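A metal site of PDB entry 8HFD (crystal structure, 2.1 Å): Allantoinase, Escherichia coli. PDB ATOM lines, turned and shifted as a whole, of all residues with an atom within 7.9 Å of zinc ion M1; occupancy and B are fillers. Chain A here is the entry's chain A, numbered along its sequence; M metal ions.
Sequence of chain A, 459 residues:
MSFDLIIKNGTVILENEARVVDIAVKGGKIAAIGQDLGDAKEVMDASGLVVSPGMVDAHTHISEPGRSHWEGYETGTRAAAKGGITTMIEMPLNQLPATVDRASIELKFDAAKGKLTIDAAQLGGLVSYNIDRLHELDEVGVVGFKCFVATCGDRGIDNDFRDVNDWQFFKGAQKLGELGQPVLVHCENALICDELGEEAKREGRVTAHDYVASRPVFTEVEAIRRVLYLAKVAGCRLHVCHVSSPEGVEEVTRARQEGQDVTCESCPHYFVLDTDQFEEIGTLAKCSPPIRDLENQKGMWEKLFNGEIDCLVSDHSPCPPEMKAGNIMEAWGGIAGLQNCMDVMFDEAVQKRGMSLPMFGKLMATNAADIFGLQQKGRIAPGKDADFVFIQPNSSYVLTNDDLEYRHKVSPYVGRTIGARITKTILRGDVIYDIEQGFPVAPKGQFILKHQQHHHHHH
A ring nitrogen (ND1) of His 59 sits at hydrogen-bond distance from the side-chain carboxylate of Glu 265 (2.7 Å).
The backbone carbonyl oxygen (O) of His 59 sits at hydrogen-bond distance from the side-chain hydroxyl (OG) of Ser 314 (3.1 Å).
OQ1 of KCX 146 lies close to a ring nitrogen (NE2) of His 61, at 3.3 Å.
N of His 61 lies close to O of His 316, at 3.3 Å.
ND1 of His 61 lies within hydrogen-bond range of O of Leu 93, 2.6 Å away.
The backbone carbonyl oxygen (O) of Asp 315 is in hydrogen-bond range of the side-chain hydroxyl (OG) of Ser 317 (2.8 Å).
NZ of KCX 146 sits close to the side-chain sulfur of Met 91.
Zinc ion M1 is bound by NE2 of His 59 (2.2 Å), NE2 of His 61 (2.2 Å) and OD1 of Asp 315 (2.4 Å).
Slightly farther from zinc ion M1 lies OQ1 of KCX 146 (2.7 Å).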
ATOM      1  N   HIS A  59       7.962 -20.770   3.951  1.00  0.00           N
ATOM      2  CA  HIS A  59       7.301 -21.099   2.697  1.00  0.00           C
ATOM      3  C   HIS A  59       6.842 -19.844   1.973  1.00  0.00           C
ATOM      4  O   HIS A  59       5.666 -19.462   2.052  1.00  0.00           O
ATOM      5  CB  HIS A  59       6.128 -22.045   3.001  1.00  0.00           C
ATOM      6  CG  HIS A  59       5.611 -22.772   1.801  1.00  0.00           C
ATOM      7  ND1 HIS A  59       5.234 -24.092   1.851  1.00  0.00           N
ATOM      8  CD2 HIS A  59       5.390 -22.352   0.532  1.00  0.00           C
ATOM      9  CE1 HIS A  59       4.786 -24.458   0.656  1.00  0.00           C
ATOM     10  NE2 HIS A  59       4.872 -23.424  -0.150  1.00  0.00           N
ATOM     11  N   THR A  60       7.761 -19.174   1.292  1.00  0.00           N
ATOM     12  CA  THR A  60       7.498 -17.915   0.612  1.00  0.00           C
ATOM     13  C   THR A  60       7.761 -18.046  -0.878  1.00  0.00           C
ATOM     14  O   THR A  60       8.857 -18.452  -1.272  1.00  0.00           O
ATOM     15  CB  THR A  60       8.377 -16.788   1.166  1.00  0.00           C
ATOM     16  OG1 THR A  60       8.457 -16.887   2.586  1.00  0.00           O
ATOM     17  CG2 THR A  60       7.786 -15.449   0.813  1.00  0.00           C
ATOM     18  N   HIS A  61       6.799 -17.622  -1.696  1.00  0.00           N
ATOM     19  CA  HIS A  61       7.018 -17.460  -3.136  1.00  0.00           C
ATOM     20  C   HIS A  61       7.223 -15.992  -3.460  1.00  0.00           C
ATOM     21  O   HIS A  61       6.304 -15.185  -3.273  1.00  0.00           O
ATOM     22  CB  HIS A  61       5.844 -18.004  -3.947  1.00  0.00           C
ATOM     23  CG  HIS A  61       5.645 -19.476  -3.779  1.00  0.00           C
ATOM     24  ND1 HIS A  61       6.479 -20.405  -4.367  1.00  0.00           N
ATOM     25  CD2 HIS A  61       4.722 -20.176  -3.083  1.00  0.00           C
ATOM     26  CE1 HIS A  61       6.080 -21.608  -4.037  1.00  0.00           C
ATOM     27  NE2 HIS A  61       5.017 -21.501  -3.262  1.00  0.00           N
ATOM     28  N   MET A  91      11.092 -20.330  -1.651  1.00  0.00           N
ATOM     29  CA  MET A  91      10.842 -21.482  -2.541  1.00  0.00           C
ATOM     30  C   MET A  91      11.569 -21.298  -3.885  1.00  0.00           C
ATOM     31  O   MET A  91      11.809 -20.154  -4.259  1.00  0.00           O
ATOM     32  CB  MET A  91       9.334 -21.582  -2.777  1.00  0.00           C
ATOM     33  CG  MET A  91       8.584 -22.172  -1.601  1.00  0.00           C
ATOM     34  SD  MET A  91       8.991 -23.915  -1.387  1.00  0.00           S
ATOM     35  CE  MET A  91       8.413 -24.183   0.292  1.00  0.00           C
ATOM     36  N   LEU A  93      10.393 -21.655  -6.776  1.00  0.00           N
ATOM     37  CA  LEU A  93       9.405 -21.233  -7.794  1.00  0.00           C
ATOM     38  C   LEU A  93       8.584 -20.074  -7.207  1.00  0.00           C
ATOM     39  O   LEU A  93       8.519 -19.986  -5.999  1.00  0.00           O
ATOM     40  CB  LEU A  93       8.517 -22.434  -8.140  1.00  0.00           C
ATOM     41  CG  LEU A  93       7.533 -22.880  -7.061  1.00  0.00           C
ATOM     42  CD1 LEU A  93       6.421 -23.728  -7.669  1.00  0.00           C
ATOM     43  CD2 LEU A  93       8.230 -23.651  -5.960  1.00  0.00           C
ATOM     44  N   ASN A  94       8.093 -19.142  -8.038  1.00  0.00           N
ATOM     45  CA  ASN A  94       7.734 -19.281  -9.476  1.00  0.00           C
ATOM     46  C   ASN A  94       8.752 -18.566 -10.374  1.00  0.00           C
ATOM     47  O   ASN A  94       8.437 -18.308 -11.535  1.00  0.00           O
ATOM     48  CB  ASN A  94       6.300 -18.787  -9.687  1.00  0.00           C
ATOM     49  CG  ASN A  94       5.320 -19.534  -8.809  1.00  0.00           C
ATOM     50  OD1 ASN A  94       5.226 -20.753  -8.879  1.00  0.00           O
ATOM     51  ND2 ASN A  94       4.588 -18.812  -7.981  1.00  0.00           N
ATOM     52  N   KCX A 146      12.671 -28.468  -2.591  1.00  0.00           N
ATOM     53  CA  KCX A 146      11.191 -28.579  -2.653  1.00  0.00           C
ATOM     54  CB  KCX A 146      10.531 -27.206  -2.508  1.00  0.00           C
ATOM     55  CG  KCX A 146       9.305 -27.177  -1.604  1.00  0.00           C
ATOM     56  CD  KCX A 146       8.166 -28.055  -2.065  1.00  0.00           C
ATOM     57  CE  KCX A 146       7.158 -27.340  -2.945  1.00  0.00           C
ATOM     58  NZ  KCX A 146       6.561 -26.193  -2.286  1.00  0.00           N
ATOM     59  C   KCX A 146      10.749 -29.251  -3.950  1.00  0.00           C
ATOM     60  O   KCX A 146      11.316 -28.920  -5.013  1.00  0.00           O
ATOM     61  CX  KCX A 146       5.378 -25.683  -2.682  1.00  0.00           C
ATOM     62  OQ1 KCX A 146       5.282 -24.756  -3.448  1.00  0.00           O
ATOM     63  OQ2 KCX A 146       4.332 -26.302  -2.159  1.00  0.00           O
ATOM     64  N   PHE A 148       7.155 -31.312  -6.152  1.00  0.00           N
ATOM     65  CA  PHE A 148       5.779 -31.763  -6.320  1.00  0.00           C
ATOM     66  C   PHE A 148       5.833 -33.161  -6.918  1.00  0.00           C
ATOM     67  O   PHE A 148       6.446 -33.360  -7.961  1.00  0.00           O
ATOM     68  CB  PHE A 148       4.986 -30.864  -7.272  1.00  0.00           C
ATOM     69  CG  PHE A 148       4.645 -29.513  -6.739  1.00  0.00           C
ATOM     70  CD1 PHE A 148       5.633 -28.609  -6.395  1.00  0.00           C
ATOM     71  CD2 PHE A 148       3.318 -29.120  -6.635  1.00  0.00           C
ATOM     72  CE1 PHE A 148       5.306 -27.338  -5.932  1.00  0.00           C
ATOM     73  CE2 PHE A 148       2.985 -27.851  -6.164  1.00  0.00           C
ATOM     74  CZ  PHE A 148       3.995 -26.964  -5.809  1.00  0.00           C
ATOM     75  N   HIS A 186       4.834 -30.766  -1.756  1.00  0.00           N
ATOM     76  CA  HIS A 186       3.415 -30.370  -1.845  1.00  0.00           C
ATOM     77  C   HIS A 186       2.679 -31.695  -2.033  1.00  0.00           C
ATOM     78  O   HIS A 186       2.827 -32.289  -3.094  1.00  0.00           O
ATOM     79  CB  HIS A 186       3.199 -29.358  -2.977  1.00  0.00           C
ATOM     80  CG  HIS A 186       1.790 -28.986  -3.235  1.00  0.00           C
ATOM     81  ND1 HIS A 186       1.364 -27.672  -3.193  1.00  0.00           N
ATOM     82  CD2 HIS A 186       0.712 -29.724  -3.577  1.00  0.00           C
ATOM     83  CE1 HIS A 186       0.081 -27.625  -3.468  1.00  0.00           C
ATOM     84  NE2 HIS A 186      -0.337 -28.866  -3.708  1.00  0.00           N
ATOM     85  N   CYS A 241       4.578 -29.995   3.419  1.00  0.00           N
ATOM     86  CA  CYS A 241       4.200 -28.592   3.281  1.00  0.00           C
ATOM     87  C   CYS A 241       2.719 -28.408   3.541  1.00  0.00           C
ATOM     88  O   CYS A 241       1.921 -29.325   3.368  1.00  0.00           O
ATOM     89  CB  CYS A 241       4.550 -28.077   1.873  1.00  0.00           C
ATOM     90  SG  CYS A 241       6.322 -27.864   1.602  1.00  0.00           S
ATOM     91  N   HIS A 242       2.353 -27.172   3.922  1.00  0.00           N
ATOM     92  CA  HIS A 242       0.986 -26.733   4.205  1.00  0.00           C
ATOM     93  C   HIS A 242      -0.052 -27.845   4.305  1.00  0.00           C
ATOM     94  O   HIS A 242      -0.783 -28.099   3.340  1.00  0.00           O
ATOM     95  CB  HIS A 242       0.530 -25.762   3.114  1.00  0.00           C
ATOM     96  CG  HIS A 242       0.866 -26.239   1.740  1.00  0.00           C
ATOM     97  ND1 HIS A 242       0.638 -27.531   1.333  1.00  0.00           N
ATOM     98  CD2 HIS A 242       1.443 -25.599   0.693  1.00  0.00           C
ATOM     99  CE1 HIS A 242       1.056 -27.673   0.089  1.00  0.00           C
ATOM    100  NE2 HIS A 242       1.550 -26.521  -0.323  1.00  0.00           N
ATOM    101  N   GLU A 265       3.979 -28.539   8.400  1.00  0.00           N
ATOM    102  CA  GLU A 265       3.652 -27.136   8.600  1.00  0.00           C
ATOM    103  C   GLU A 265       2.205 -26.948   8.190  1.00  0.00           C
ATOM    104  O   GLU A 265       1.614 -27.828   7.539  1.00  0.00           O
ATOM    105  CB  GLU A 265       4.577 -26.216   7.773  1.00  0.00           C
ATOM    106  CG  GLU A 265       4.060 -26.066   6.333  1.00  0.00           C
ATOM    107  CD  GLU A 265       5.099 -25.601   5.307  1.00  0.00           C
ATOM    108  OE1 GLU A 265       6.271 -25.323   5.655  1.00  0.00           O
ATOM    109  OE2 GLU A 265       4.697 -25.495   4.116  1.00  0.00           O
ATOM    110  N   CYS A 267      -0.767 -23.278   7.454  1.00  0.00           N
ATOM    111  CA  CYS A 267      -0.807 -21.852   7.154  1.00  0.00           C
ATOM    112  C   CYS A 267      -1.961 -21.181   7.887  1.00  0.00           C
ATOM    113  O   CYS A 267      -2.947 -21.834   8.235  1.00  0.00           O
ATOM    114  CB  CYS A 267      -0.940 -21.600   5.637  1.00  0.00           C
ATOM    115  SG  CYS A 267       0.229 -22.571   4.602  1.00  0.00           S
ATOM    116  N   SER A 288      -4.395 -24.269  -3.400  1.00  0.00           N
ATOM    117  CA  SER A 288      -4.232 -25.670  -3.867  1.00  0.00           C
ATOM    118  C   SER A 288      -4.651 -26.623  -2.774  1.00  0.00           C
ATOM    119  O   SER A 288      -5.719 -27.207  -2.952  1.00  0.00           O
ATOM    120  CB  SER A 288      -2.858 -25.981  -4.409  1.00  0.00           C
ATOM    121  OG  SER A 288      -2.782 -27.300  -4.902  1.00  0.00           O
ATOM    122  N   PRO A 289      -3.913 -26.836  -1.666  1.00  0.00           N
ATOM    123  CA  PRO A 289      -4.466 -27.638  -0.616  1.00  0.00           C
ATOM    124  C   PRO A 289      -5.628 -26.674  -0.297  1.00  0.00           C
ATOM    125  O   PRO A 289      -5.390 -25.542   0.007  1.00  0.00           O
ATOM    126  CB  PRO A 289      -3.362 -27.769   0.448  1.00  0.00           C
ATOM    127  CG  PRO A 289      -2.140 -27.163  -0.207  1.00  0.00           C
ATOM    128  CD  PRO A 289      -2.613 -26.268  -1.326  1.00  0.00           C
ATOM    129  N   VAL A 313       3.415 -21.144   8.342  1.00  0.00           N
ATOM    130  CA  VAL A 313       4.106 -20.462   7.208  1.00  0.00           C
ATOM    131  C   VAL A 313       3.058 -19.751   6.350  1.00  0.00           C
ATOM    132  O   VAL A 313       1.871 -20.020   6.518  1.00  0.00           O
ATOM    133  CB  VAL A 313       4.902 -21.483   6.392  1.00  0.00           C
ATOM    134  CG1 VAL A 313       5.931 -22.213   7.234  1.00  0.00           C
ATOM    135  CG2 VAL A 313       3.979 -22.467   5.682  1.00  0.00           C
ATOM    136  N   SER A 314       3.500 -18.883   5.437  1.00  0.00           N
ATOM    137  CA  SER A 314       2.523 -18.095   4.691  1.00  0.00           C
ATOM    138  C   SER A 314       1.976 -18.867   3.510  1.00  0.00           C
ATOM    139  O   SER A 314       0.783 -18.781   3.219  1.00  0.00           O
ATOM    140  CB  SER A 314       3.126 -16.792   4.178  1.00  0.00           C
ATOM    141  OG  SER A 314       4.135 -17.042   3.238  1.00  0.00           O
ATOM    142  N   ASP A 315       2.827 -19.633   2.837  1.00  0.00           N
ATOM    143  CA  ASP A 315       2.578 -20.039   1.447  1.00  0.00           C
ATOM    144  C   ASP A 315       2.113 -18.859   0.616  1.00  0.00           C
ATOM    145  O   ASP A 315       1.159 -18.955  -0.168  1.00  0.00           O
ATOM    146  CB  ASP A 315       1.580 -21.195   1.343  1.00  0.00           C
ATOM    147  CG  ASP A 315       1.554 -21.798  -0.066  1.00  0.00           C
ATOM    148  OD1 ASP A 315       2.461 -21.460  -0.879  1.00  0.00           O
ATOM    149  OD2 ASP A 315       0.647 -22.598  -0.357  1.00  0.00           O
ATOM    150  N   HIS A 316       2.793 -17.710   0.812  1.00  0.00           N
ATOM    151  CA  HIS A 316       2.467 -16.514   0.053  1.00  0.00           C
ATOM    152  C   HIS A 316       2.509 -16.847  -1.434  1.00  0.00           C
ATOM    153  O   HIS A 316       3.570 -17.195  -1.971  1.00  0.00           O
ATOM    154  CB  HIS A 316       3.449 -15.376   0.385  1.00  0.00           C
ATOM    155  CG  HIS A 316       3.133 -14.073  -0.283  1.00  0.00           C
ATOM    156  ND1 HIS A 316       1.922 -13.434  -0.119  1.00  0.00           N
ATOM    157  CD2 HIS A 316       3.864 -13.304  -1.114  1.00  0.00           C
ATOM    158  CE1 HIS A 316       1.927 -12.317  -0.825  1.00  0.00           C
ATOM    159  NE2 HIS A 316       3.090 -12.203  -1.435  1.00  0.00           N
ATOM    160  N   SER A 317       1.356 -16.745  -2.085  1.00  0.00           N
ATOM    161  CA  SER A 317       1.175 -17.208  -3.454  1.00  0.00           C
ATOM    162  C   SER A 317       0.406 -16.166  -4.261  1.00  0.00           C
ATOM    163  O   SER A 317      -0.718 -16.398  -4.689  1.00  0.00           O
ATOM    164  CB  SER A 317       0.447 -18.555  -3.472  1.00  0.00           C
ATOM    165  OG  SER A 317       1.236 -19.566  -2.877  1.00  0.00           O
HETATM  166 ZN    ZN M   1       3.841 -22.961  -2.065  1.00  0.00          ZN
HETATM  167 ZN    ZN M   2       2.358 -26.001  -2.306  1.00  0.00          ZN
